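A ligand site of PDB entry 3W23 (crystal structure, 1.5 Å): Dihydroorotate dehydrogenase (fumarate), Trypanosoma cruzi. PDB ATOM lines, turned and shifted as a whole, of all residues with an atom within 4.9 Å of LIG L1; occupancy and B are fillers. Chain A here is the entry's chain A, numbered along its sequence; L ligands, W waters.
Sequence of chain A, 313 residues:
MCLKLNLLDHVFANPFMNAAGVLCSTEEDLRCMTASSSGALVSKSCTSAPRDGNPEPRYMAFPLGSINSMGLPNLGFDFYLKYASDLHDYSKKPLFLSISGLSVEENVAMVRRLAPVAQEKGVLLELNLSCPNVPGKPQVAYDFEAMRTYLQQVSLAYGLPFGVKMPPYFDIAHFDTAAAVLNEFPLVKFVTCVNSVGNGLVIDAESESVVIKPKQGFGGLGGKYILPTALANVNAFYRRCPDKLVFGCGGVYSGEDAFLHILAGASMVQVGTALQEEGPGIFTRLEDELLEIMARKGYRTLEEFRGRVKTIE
Ala 19 touches LIG L1 (CB to O3, 3.2 Å). CA of Gly 21 touches N3 of LIG L1 (3.4 Å). CD1 of Tyr 59 touches C7 of LIG L1, 3.7 Å away. ND2 of Asn 68 touches C8 of LIG L1, 3.5 Å away. SD of Met 70 touches C7 of LIG L1 (3.8 Å). Ser 196 touches LIG L1. C of Gly 222 touches O8 of LIG L1 (3.7 Å). Ile 226 touches LIG L1. CA of Gly 250 touches O8 of LIG L1, at 3.4 Å. C of Val 271 touches O7 of LIG L1 (3.9 Å). Hydrophobic or aromatic side chains that line LIG L1: Ala 19, Ala 20, Tyr 59, Met 70 and Ile 226. 22 residues have an atom within 4 Å of LIG L1: Ala 19, Ala 20, Gly 21, Lys 44, Ser 45, Tyr 59, Asn 68, Met 70, Asn 128, Lys 165, Val 194, Asn 195, Ser 196, Gly 222, Gly 223, Ile 226, Cys 249, Gly 250, Gly 251, Val 271, Gly 272 and Thr 273. Along chain A the residues within 4 Å of LIG L1 span positions 19 to 273.
The side-chain sulfur of Cys 249 sits at hydrogen-bond distance from the side-chain amide oxygen of Gln 270 (3.7 Å). N of Ala 19 lies within hydrogen-bond range of O of Val 271 (3.0 Å). OG of Ser 196 sits at hydrogen-bond distance from OD1 of Asn 195 (3.5 Å). The side-chain hydroxyl (OG) of Ser 98 lies within hydrogen-bond range of the side-chain hydroxyl (OG) of Ser 45, at 2.5 Å. O of Gly 222 sits at hydrogen-bond distance from N of Ser 66, at 3.0 Å. The side-chain amide nitrogen of Asn 195 sits at hydrogen-bond distance from the side-chain amide oxygen of Asn 128, 3.3 Å away. The backbone NH (N) of Met 70 is in hydrogen-bond range of the side-chain amide oxygen (OD1) of Asn 68 (3.3 Å). The side-chain hydroxyl of Thr 273 sits at hydrogen-bond distance from the side-chain hydroxyl of Ser 66, 2.7 Å away.
Water W1 lies within hydrogen-bond range of O7 of LIG L1 (2.7 Å), N of Ala 274 (2.9 Å), O of Val 252 (2.9 Å) and N of Thr 273 (3.5 Å). Water W3 lies within hydrogen-bond range of OG of Ser 98 (2.6 Å), OE1 of Glu 126 (2.7 Å) and O1 of LIG L1 (2.8 Å).
A nitrogen (N1) of LIG L1 sits close to a nitrogen (N2) of LG2 L2, at 3.5 Å.
The backbone carbonyl oxygen (O) of Ala 20 is in hydrogen-bond range of an oxygen (O3) of LIG L1, at 2.8 Å. An oxygen (O7) of LIG L1 sits at hydrogen-bond distance from the backbone NH (N) of Gly 272 (2.8 Å). An oxygen (O1) of LIG L1 is in hydrogen-bond range of the side-chain amide nitrogen (ND2) of Asn 195. N of Gly 251 is in hydrogen-bond range of O8 of LIG L1, 2.8 Å away. OG of Ser 45 sits at hydrogen-bond distance from N2 of LIG L1, 2.8 Å away. The backbone NH (N) of Thr 273 sits at hydrogen-bond distance from an oxygen (O9) of LIG L1, 2.8 Å away. The backbone carbonyl oxygen of Val 194 lies within hydrogen-bond range of an oxygen (O4) of LIG L1 (2.9 Å). The side-chain amide nitrogen (ND2) of Asn 128 sits at hydrogen-bond distance from an oxygen (O4) of LG2 L2, 2.9 Å away. O2 of LIG L1 lies within hydrogen-bond range of NZ of Lys 44 (2.7 Å). The side-chain amide oxygen (OD1) of Asn 195 is in hydrogen-bond range of a nitrogen (N2) of LG2 L2 (2.8 Å). O8 of LIG L1 sits at hydrogen-bond distance from N of Gly 223. O1 of LIG L1 sits at hydrogen-bond distance from ND2 of Asn 128, at 3.5 Å. The side-chain amino group of Lys 165 sits at hydrogen-bond distance from an oxygen (O3) of LIG L1 (2.8 Å). O2 of LG2 L2 is in hydrogen-bond range of N of Leu 72, 2.9 Å away. The side-chain amino group (NZ) of Lys 44 lies within salt-bridge range of an oxygen (O2) of LG2 L2, at 3.3 Å. The side-chain sulfur of Cys 249 sits at hydrogen-bond distance from an oxygen (O4) of LIG L1 (3.4 Å). ND2 of Asn 68 sits at hydrogen-bond distance from O3 of LG2 L2, at 2.9 Å. The backbone NH of Met 70 sits at hydrogen-bond distance from an oxygen (O1) of LG2 L2 (3.1 Å). The side-chain hydroxyl (OG) of Ser 196 sits at hydrogen-bond distance from an oxygen (O3) of LG2 L2 (2.8 Å). The side-chain hydroxyl (OG1) of Thr 273 is in hydrogen-bond range of an oxygen (O9) of LIG L1, 2.6 Å away.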
ATOM      1  N   ALA A  19     -24.071  18.572  -4.478  1.00  0.00           N
ATOM      2  CA  ALA A  19     -23.457  18.207  -3.237  1.00  0.00           C
ATOM      3  C   ALA A  19     -23.934  16.878  -2.730  1.00  0.00           C
ATOM      4  O   ALA A  19     -25.078  16.504  -2.962  1.00  0.00           O
ATOM      5  CB  ALA A  19     -23.828  19.288  -2.180  1.00  0.00           C
ATOM      6  N   ALA A  20     -23.064  16.062  -2.174  1.00  0.00           N
ATOM      7  CA  ALA A  20     -23.477  14.760  -1.679  1.00  0.00           C
ATOM      8  C   ALA A  20     -24.708  14.905  -0.779  1.00  0.00           C
ATOM      9  O   ALA A  20     -24.785  15.793   0.053  1.00  0.00           O
ATOM     10  CB  ALA A  20     -22.338  14.060  -0.950  1.00  0.00           C
ATOM     11  N   GLY A  21     -25.648  13.981  -0.958  1.00  0.00           N
ATOM     12  CA  GLY A  21     -26.858  13.952  -0.268  1.00  0.00           C
ATOM     13  C   GLY A  21     -28.027  14.486  -0.974  1.00  0.00           C
ATOM     14  O   GLY A  21     -29.130  14.174  -0.646  1.00  0.00           O
ATOM     15  N   VAL A  22     -27.804  15.370  -1.915  1.00  0.00           N
ATOM     16  CA  VAL A  22     -28.936  16.026  -2.659  1.00  0.00           C
ATOM     17  C   VAL A  22     -29.057  15.399  -4.029  1.00  0.00           C
ATOM     18  O   VAL A  22     -28.081  15.357  -4.782  1.00  0.00           O
ATOM     19  CB  VAL A  22     -28.671  17.554  -2.721  1.00  0.00           C
ATOM     20  CG1 VAL A  22     -29.711  18.219  -3.550  1.00  0.00           C
ATOM     21  CG2 VAL A  22     -28.648  18.066  -1.289  1.00  0.00           C
ATOM     22  N   LYS A  44     -24.950   9.658  -3.095  1.00  0.00           N
ATOM     23  CA  LYS A  44     -25.242   9.782  -1.673  1.00  0.00           C
ATOM     24  C   LYS A  44     -24.188   9.055  -0.813  1.00  0.00           C
ATOM     25  O   LYS A  44     -23.952   7.873  -1.091  1.00  0.00           O
ATOM     26  CB  LYS A  44     -26.633   9.188  -1.381  1.00  0.00           C
ATOM     27  CG  LYS A  44     -27.005   9.157   0.080  1.00  0.00           C
ATOM     28  CD  LYS A  44     -27.171  10.531   0.861  1.00  0.00           C
ATOM     29  CE  LYS A  44     -27.163  10.420   2.412  1.00  0.00           C
ATOM     30  NZ  LYS A  44     -27.339  11.684   3.301  1.00  0.00           N
ATOM     31  N   SER A  45     -23.735   9.728   0.240  1.00  0.00           N
ATOM     32  CA  SER A  45     -22.750   9.064   1.171  1.00  0.00           C
ATOM     33  C   SER A  45     -23.416   7.793   1.650  1.00  0.00           C
ATOM     34  O   SER A  45     -24.554   7.746   2.016  1.00  0.00           O
ATOM     35  CB  SER A  45     -22.455   9.892   2.379  1.00  0.00           C
ATOM     36  OG  SER A  45     -21.744  11.039   1.947  1.00  0.00           O
ATOM     37  N   TYR A  59     -35.493  17.337   7.188  1.00  0.00           N
ATOM     38  CA  TYR A  59     -34.933  18.412   6.355  1.00  0.00           C
ATOM     39  C   TYR A  59     -36.016  19.462   6.278  1.00  0.00           C
ATOM     40  O   TYR A  59     -37.177  19.167   5.959  1.00  0.00           O
ATOM     41  CB  TYR A  59     -34.599  17.891   4.925  1.00  0.00           C
ATOM     42  CG  TYR A  59     -34.269  18.974   3.882  1.00  0.00           C
ATOM     43  CD1 TYR A  59     -33.006  19.509   3.760  1.00  0.00           C
ATOM     44  CD2 TYR A  59     -35.278  19.499   3.122  1.00  0.00           C
ATOM     45  CE1 TYR A  59     -32.721  20.519   2.900  1.00  0.00           C
ATOM     46  CE2 TYR A  59     -35.051  20.578   2.289  1.00  0.00           C
ATOM     47  CZ  TYR A  59     -33.736  21.062   2.129  1.00  0.00           C
ATOM     48  OH  TYR A  59     -33.410  22.043   1.195  1.00  0.00           O
ATOM     49  N   SER A  66     -31.153  25.924   4.731  1.00  0.00           N
ATOM     50  CA  SER A  66     -31.735  24.691   5.145  1.00  0.00           C
ATOM     51  C   SER A  66     -31.080  24.180   6.416  1.00  0.00           C
ATOM     52  O   SER A  66     -30.003  24.536   6.822  1.00  0.00           O
ATOM     53  CB  SER A  66     -31.606  23.621   4.039  1.00  0.00           C
ATOM     54  OG  SER A  66     -30.234  23.228   3.905  1.00  0.00           O
ATOM     55  N   ASN A  68     -30.807  20.164   8.416  1.00  0.00           N
ATOM     56  CA  ASN A  68     -31.062  18.725   8.223  1.00  0.00           C
ATOM     57  C   ASN A  68     -30.421  17.916   9.335  1.00  0.00           C
ATOM     58  O   ASN A  68     -29.315  18.160   9.763  1.00  0.00           O
ATOM     59  CB  ASN A  68     -30.646  18.178   6.835  1.00  0.00           C
ATOM     60  CG  ASN A  68     -29.212  17.784   6.770  1.00  0.00           C
ATOM     61  OD1 ASN A  68     -28.865  16.658   7.163  1.00  0.00           O
ATOM     62  ND2 ASN A  68     -28.367  18.653   6.298  1.00  0.00           N
ATOM     63  N   MET A  70     -30.572  14.171   8.605  1.00  0.00           N
ATOM     64  CA  MET A  70     -31.105  13.081   7.834  1.00  0.00           C
ATOM     65  C   MET A  70     -30.807  11.719   8.481  1.00  0.00           C
ATOM     66  O   MET A  70     -31.594  10.787   8.422  1.00  0.00           O
ATOM     67  CB  MET A  70     -30.485  13.082   6.469  1.00  0.00           C
ATOM     68  CG  MET A  70     -30.734  14.301   5.627  1.00  0.00           C
ATOM     69  SD  MET A  70     -32.420  14.760   5.378  1.00  0.00           S
ATOM     70  CE  MET A  70     -32.983  13.476   4.329  1.00  0.00           C
ATOM     71  N   LEU A  72     -28.133   9.818   7.649  1.00  0.00           N
ATOM     72  CA  LEU A  72     -27.468   9.053   6.632  1.00  0.00           C
ATOM     73  C   LEU A  72     -28.393   7.969   6.007  1.00  0.00           C
ATOM     74  O   LEU A  72     -27.980   6.788   5.811  1.00  0.00           O
ATOM     75  CB  LEU A  72     -26.119   8.515   7.137  1.00  0.00           C
ATOM     76  CG  LEU A  72     -24.988   7.966   6.263  1.00  0.00           C
ATOM     77  CD1 LEU A  72     -24.759   8.915   5.157  1.00  0.00           C
ATOM     78  CD2 LEU A  72     -23.758   7.809   7.147  1.00  0.00           C
ATOM     79  N   SER A  98     -19.476   8.912  -2.899  1.00  0.00           N
ATOM     80  CA  SER A  98     -19.167   9.347  -1.571  1.00  0.00           C
ATOM     81  C   SER A  98     -19.413   8.201  -0.579  1.00  0.00           C
ATOM     82  O   SER A  98     -20.423   7.465  -0.640  1.00  0.00           O
ATOM     83  CB  SER A  98     -20.066  10.478  -1.150  1.00  0.00           C
ATOM     84  OG  SER A  98     -19.868  10.818   0.237  1.00  0.00           O
ATOM     85  N   GLU A 126     -15.042  10.249  -2.942  1.00  0.00           N
ATOM     86  CA  GLU A 126     -15.111  11.289  -1.936  1.00  0.00           C
ATOM     87  C   GLU A 126     -15.405  10.672  -0.583  1.00  0.00           C
ATOM     88  O   GLU A 126     -16.493  10.212  -0.323  1.00  0.00           O
ATOM     89  CB  GLU A 126     -16.141  12.387  -2.361  1.00  0.00           C
ATOM     90  CG  GLU A 126     -16.130  13.607  -1.427  1.00  0.00           C
ATOM     91  CD  GLU A 126     -17.150  14.708  -1.824  1.00  0.00           C
ATOM     92  OE1 GLU A 126     -18.308  14.586  -1.395  1.00  0.00           O
ATOM     93  OE2 GLU A 126     -16.783  15.687  -2.498  1.00  0.00           O
ATOM     94  N   ASN A 128     -16.262  11.083   3.200  1.00  0.00           N
ATOM     95  CA  ASN A 128     -16.854  12.035   4.126  1.00  0.00           C
ATOM     96  C   ASN A 128     -16.265  11.938   5.469  1.00  0.00           C
ATOM     97  O   ASN A 128     -16.488  10.962   6.158  1.00  0.00           O
ATOM     98  CB  ASN A 128     -18.358  11.853   4.143  1.00  0.00           C
ATOM     99  CG  ASN A 128     -19.042  12.866   4.998  1.00  0.00           C
ATOM    100  OD1 ASN A 128     -18.536  13.906   5.296  1.00  0.00           O
ATOM    101  ND2 ASN A 128     -20.319  12.645   5.127  1.00  0.00           N
ATOM    102  N   LYS A 165     -14.292  15.112   2.023  1.00  0.00           N
ATOM    103  CA  LYS A 165     -15.315  16.116   2.306  1.00  0.00           C
ATOM    104  C   LYS A 165     -15.108  16.549   3.735  1.00  0.00           C
ATOM    105  O   LYS A 165     -15.154  15.718   4.680  1.00  0.00           O
ATOM    106  CB  LYS A 165     -16.693  15.528   2.149  1.00  0.00           C
ATOM    107  CG  LYS A 165     -17.878  16.453   2.458  1.00  0.00           C
ATOM    108  CD  LYS A 165     -18.106  17.511   1.401  1.00  0.00           C
ATOM    109  CE  LYS A 165     -19.416  18.198   1.542  1.00  0.00           C
ATOM    110  NZ  LYS A 165     -20.574  17.384   1.217  1.00  0.00           N
ATOM    111  N   VAL A 194     -17.386  23.060   1.913  1.00  0.00           N
ATOM    112  CA  VAL A 194     -17.570  22.449   3.214  1.00  0.00           C
ATOM    113  C   VAL A 194     -18.865  21.650   3.288  1.00  0.00           C
ATOM    114  O   VAL A 194     -19.751  21.803   2.518  1.00  0.00           O
ATOM    115  CB  VAL A 194     -17.648  23.516   4.348  1.00  0.00           C
ATOM    116  CG1 VAL A 194     -16.315  24.202   4.505  1.00  0.00           C
ATOM    117  CG2 VAL A 194     -18.747  24.534   4.095  1.00  0.00           C
ATOM    118  N   ASN A 195     -18.894  20.755   4.242  1.00  0.00           N
ATOM    119  CA  ASN A 195     -20.116  20.126   4.720  1.00  0.00           C
ATOM    120  C   ASN A 195     -20.933  21.193   5.495  1.00  0.00           C
ATOM    121  O   ASN A 195     -20.513  22.267   5.616  1.00  0.00           O
ATOM    122  CB  ASN A 195     -19.803  18.858   5.567  1.00  0.00           C
ATOM    123  CG  ASN A 195     -20.849  17.749   5.412  1.00  0.00           C
ATOM    124  OD1 ASN A 195     -21.989  18.004   5.519  1.00  0.00           O
ATOM    125  ND2 ASN A 195     -20.402  16.571   5.102  1.00  0.00           N
ATOM    126  N   SER A 196     -22.107  20.805   5.945  1.00  0.00           N
ATOM    127  CA  SER A 196     -22.965  21.731   6.632  1.00  0.00           C
ATOM    128  C   SER A 196     -22.356  22.289   7.919  1.00  0.00           C
ATOM    129  O   SER A 196     -21.524  21.718   8.482  1.00  0.00           O
ATOM    130  CB  SER A 196     -24.338  21.073   6.898  1.00  0.00           C
ATOM    131  OG  SER A 196     -24.234  19.840   7.404  1.00  0.00           O
ATOM    132  N   GLY A 222     -27.200  24.601   5.776  1.00  0.00           N
ATOM    133  CA  GLY A 222     -26.757  24.926   4.457  1.00  0.00           C
ATOM    134  C   GLY A 222     -27.380  26.168   3.921  1.00  0.00           C
ATOM    135  O   GLY A 222     -28.295  26.737   4.519  1.00  0.00           O
ATOM    136  N   GLY A 223     -26.909  26.567   2.768  1.00  0.00           N
ATOM    137  CA  GLY A 223     -27.503  27.654   2.067  1.00  0.00           C
ATOM    138  C   GLY A 223     -26.912  29.034   2.294  1.00  0.00           C
ATOM    139  O   GLY A 223     -25.702  29.115   2.588  1.00  0.00           O
ATOM    140  N   ILE A 226     -24.330  30.103   5.112  1.00  0.00           N
ATOM    141  CA  ILE A 226     -23.004  29.546   5.242  1.00  0.00           C
ATOM    142  C   ILE A 226     -22.044  29.971   4.114  1.00  0.00           C
ATOM    143  O   ILE A 226     -20.892  29.549   4.196  1.00  0.00           O
ATOM    144  CB  ILE A 226     -23.030  27.972   5.341  1.00  0.00           C
ATOM    145  CG1 ILE A 226     -23.239  27.272   3.987  1.00  0.00           C
ATOM    146  CG2 ILE A 226     -24.057  27.502   6.342  1.00  0.00           C
ATOM    147  CD1 ILE A 226     -22.793  25.815   4.092  1.00  0.00           C
ATOM    148  N   CYS A 249     -18.105  24.010  -1.791  1.00  0.00           N
ATOM    149  CA  CYS A 249     -19.494  23.654  -1.492  1.00  0.00           C
ATOM    150  C   CYS A 249     -19.994  24.592  -0.379  1.00  0.00           C
ATOM    151  O   CYS A 249     -19.313  24.739   0.611  1.00  0.00           O
ATOM    152  CB  CYS A 249     -19.609  22.201  -1.079  1.00  0.00           C
ATOM    153  SG  CYS A 249     -21.280  21.599  -0.898  1.00  0.00           S
ATOM    154  N   GLY A 250     -21.147  25.208  -0.569  1.00  0.00           N
ATOM    155  CA  GLY A 250     -21.806  25.980   0.484  1.00  0.00           C
ATOM    156  C   GLY A 250     -22.301  27.288  -0.032  1.00  0.00           C
ATOM    157  O   GLY A 250     -21.544  28.135  -0.495  1.00  0.00           O
ATOM    158  N   GLY A 251     -23.627  27.433   0.065  1.00  0.00           N
ATOM    159  CA  GLY A 251     -24.220  28.695  -0.249  1.00  0.00           C
ATOM    160  C   GLY A 251     -24.250  29.085  -1.689  1.00  0.00           C
ATOM    161  O   GLY A 251     -24.506  30.277  -1.999  1.00  0.00           O
ATOM    162  N   VAL A 252     -24.140  28.138  -2.636  1.00  0.00           N
ATOM    163  CA  VAL A 252     -24.216  28.500  -4.067  1.00  0.00           C
ATOM    164  C   VAL A 252     -25.670  28.472  -4.511  1.00  0.00           C
ATOM    165  O   VAL A 252     -26.294  27.452  -4.557  1.00  0.00           O
ATOM    166  CB  VAL A 252     -23.359  27.544  -4.946  1.00  0.00           C
ATOM    167  CG1 VAL A 252     -23.555  27.923  -6.399  1.00  0.00           C
ATOM    168  CG2 VAL A 252     -21.893  27.638  -4.508  1.00  0.00           C
ATOM    169  N   GLN A 270     -19.961  22.642  -5.876  1.00  0.00           N
ATOM    170  CA  GLN A 270     -21.096  21.737  -5.582  1.00  0.00           C
ATOM    171  C   GLN A 270     -22.265  22.579  -5.041  1.00  0.00           C
ATOM    172  O   GLN A 270     -22.048  23.639  -4.415  1.00  0.00           O
ATOM    173  CB  GLN A 270     -20.655  20.741  -4.482  1.00  0.00           C
ATOM    174  CG  GLN A 270     -19.344  20.021  -4.765  1.00  0.00           C
ATOM    175  CD  GLN A 270     -19.106  18.859  -3.855  1.00  0.00           C
ATOM    176  OE1 GLN A 270     -19.580  18.893  -2.724  1.00  0.00           O
ATOM    177  NE2 GLN A 270     -18.311  17.883  -4.259  1.00  0.00           N
ATOM    178  N   VAL A 271     -23.448  22.073  -5.316  1.00  0.00           N
ATOM    179  CA  VAL A 271     -24.714  22.761  -5.081  1.00  0.00           C
ATOM    180  C   VAL A 271     -25.618  21.836  -4.261  1.00  0.00           C
ATOM    181  O   VAL A 271     -26.007  20.778  -4.789  1.00  0.00           O
ATOM    182  CB  VAL A 271     -25.367  23.207  -6.362  1.00  0.00           C
ATOM    183  CG1 VAL A 271     -26.534  24.055  -6.038  1.00  0.00           C
ATOM    184  CG2 VAL A 271     -24.375  23.916  -7.292  1.00  0.00           C
ATOM    185  N   GLY A 272     -25.934  22.200  -3.038  1.00  0.00           N
ATOM    186  CA  GLY A 272     -26.765  21.405  -2.108  1.00  0.00           C
ATOM    187  C   GLY A 272     -28.160  22.045  -2.020  1.00  0.00           C
ATOM    188  O   GLY A 272     -29.029  21.720  -2.828  1.00  0.00           O
ATOM    189  N   THR A 273     -28.342  22.829  -0.942  1.00  0.00           N
ATOM    190  CA  THR A 273     -29.628  23.405  -0.699  1.00  0.00           C
ATOM    191  C   THR A 273     -30.353  23.979  -1.899  1.00  0.00           C
ATOM    192  O   THR A 273     -31.508  23.741  -2.152  1.00  0.00           O
ATOM    193  CB  THR A 273     -29.504  24.482   0.385  1.00  0.00           C
ATOM    194  OG1 THR A 273     -28.957  23.881   1.571  1.00  0.00           O
ATOM    195  CG2 THR A 273     -30.820  25.116   0.721  1.00  0.00           C
ATOM    196  N   ALA A 274     -29.618  24.780  -2.691  1.00  0.00           N
ATOM    197  CA  ALA A 274     -30.292  25.464  -3.810  1.00  0.00           C
ATOM    198  C   ALA A 274     -30.786  24.493  -4.844  1.00  0.00           C
ATOM    199  O   ALA A 274     -31.795  24.711  -5.477  1.00  0.00           O
ATOM    200  CB  ALA A 274     -29.342  26.459  -4.416  1.00  0.00           C
HETATM  201  N1  LIG L   1     -22.821  15.851   2.789  1.00  0.00           N
HETATM  202  C1  LIG L   1     -22.186  14.636   2.641  1.00  0.00           C
HETATM  203  O1  LIG L   1     -20.966  14.716   2.391  1.00  0.00           O
HETATM  204  N2  LIG L   1     -22.843  13.490   2.589  1.00  0.00           N
HETATM  205  C2  LIG L   1     -24.162  13.402   2.694  1.00  0.00           C
HETATM  206  O2  LIG L   1     -24.765  12.304   2.604  1.00  0.00           O
HETATM  207  C3  LIG L   1     -24.882  14.591   2.937  1.00  0.00           C
HETATM  208  N3  LIG L   1     -26.226  14.574   3.013  1.00  0.00           N
HETATM  209  C4  LIG L   1     -26.951  15.741   2.892  1.00  0.00           C
HETATM  210  C5  LIG L   1     -28.343  15.715   2.851  1.00  0.00           C
HETATM  211  C6  LIG L   1     -29.060  16.899   2.812  1.00  0.00           C
HETATM  212  C7  LIG L   1     -30.590  16.866   2.747  1.00  0.00           C
HETATM  213  C8  LIG L   1     -28.371  18.124   2.792  1.00  0.00           C
HETATM  214  C9  LIG L   1     -29.110  19.439   2.739  1.00  0.00           C
HETATM  215  C10 LIG L   1     -26.993  18.185   2.884  1.00  0.00           C
HETATM  216  C11 LIG L   1     -26.281  17.017   2.927  1.00  0.00           C
HETATM  217  N4  LIG L   1     -24.852  17.014   2.987  1.00  0.00           N
HETATM  218  C12 LIG L   1     -24.152  15.811   2.881  1.00  0.00           C
HETATM  219  C13 LIG L   1     -24.153  18.306   2.983  1.00  0.00           C
HETATM  220  C14 LIG L   1     -24.060  18.914   1.622  1.00  0.00           C
HETATM  221  O3  LIG L   1     -23.292  18.039   0.761  1.00  0.00           O
HETATM  222  C15 LIG L   1     -23.389  20.242   1.613  1.00  0.00           C
HETATM  223  O4  LIG L   1     -22.037  20.055   2.084  1.00  0.00           O
HETATM  224  C16 LIG L   1     -24.078  21.255   2.549  1.00  0.00           C
HETATM  225  O5  LIG L   1     -25.522  21.124   2.340  1.00  0.00           O
HETATM  226  C17 LIG L   1     -23.671  22.683   2.219  1.00  0.00           C
HETATM  227  O6  LIG L   1     -23.923  23.051   0.859  1.00  0.00           O
HETATM  228  P1  LIG L   1     -25.191  24.015   0.464  1.00  0.00           P
HETATM  229  O7  LIG L   1     -25.172  24.093  -1.060  1.00  0.00           O
HETATM  230  O8  LIG L   1     -25.017  25.318   1.227  1.00  0.00           O
HETATM  231  O9  LIG L   1     -26.442  23.267   1.008  1.00  0.00           O
HETATM  232  O1  LG2 L   2     -27.514  13.750   8.272  1.00  0.00           O
HETATM  233  C1  LG2 L   2     -26.947  13.234   7.300  1.00  0.00           C
HETATM  234  O2  LG2 L   2     -27.158  12.274   6.579  1.00  0.00           O
HETATM  235  C2  LG2 L   2     -25.821  14.179   6.782  1.00  0.00           C
HETATM  236  N1  LG2 L   2     -26.205  15.541   6.603  1.00  0.00           N
HETATM  237  C3  LG2 L   2     -25.295  16.544   6.271  1.00  0.00           C
HETATM  238  O3  LG2 L   2     -25.617  17.741   6.175  1.00  0.00           O
HETATM  239  N2  LG2 L   2     -24.028  16.120   6.032  1.00  0.00           N
HETATM  240  C4  LG2 L   2     -23.568  14.792   6.132  1.00  0.00           C
HETATM  241  O4  LG2 L   2     -22.366  14.557   5.895  1.00  0.00           O
HETATM  242  C5  LG2 L   2     -24.535  13.818   6.506  1.00  0.00           C
HETATM  243  C6  LG2 L   2     -24.050  12.481   6.658  1.00  0.00           C
HETATM  244  C7  LG2 L   2     -23.182  12.232   8.016  1.00  0.00           C
HETATM  245  C8  LG2 L   2     -23.924  12.095   9.104  1.00  0.00           C
HETATM  246  C9  LG2 L   2     -24.326  10.800   9.519  1.00  0.00           C
HETATM  247  C10 LG2 L   2     -25.125  10.793  10.671  1.00  0.00           C
HETATM  248 CL1  LG2 L   2     -25.748   9.196  11.189  1.00  0.00          CL
HETATM  249  C11 LG2 L   2     -25.509  11.933  11.399  1.00  0.00           C
HETATM  250  C12 LG2 L   2     -25.045  13.167  11.017  1.00  0.00           C
HETATM  251  C13 LG2 L   2     -24.207  13.257   9.878  1.00  0.00           C
HETATM  252  O   HOH W   1     -26.970  25.769  -2.244  1.00  0.00           O
HETATM  253  O   HOH W   2     -26.389  21.197   4.823  1.00  0.00           O
HETATM  254  O   HOH W   3     -19.100  13.274   0.825  1.00  0.00           O
HETATM  255  O   HOH W   4     -23.234  25.228  -2.516  1.00  0.00           O
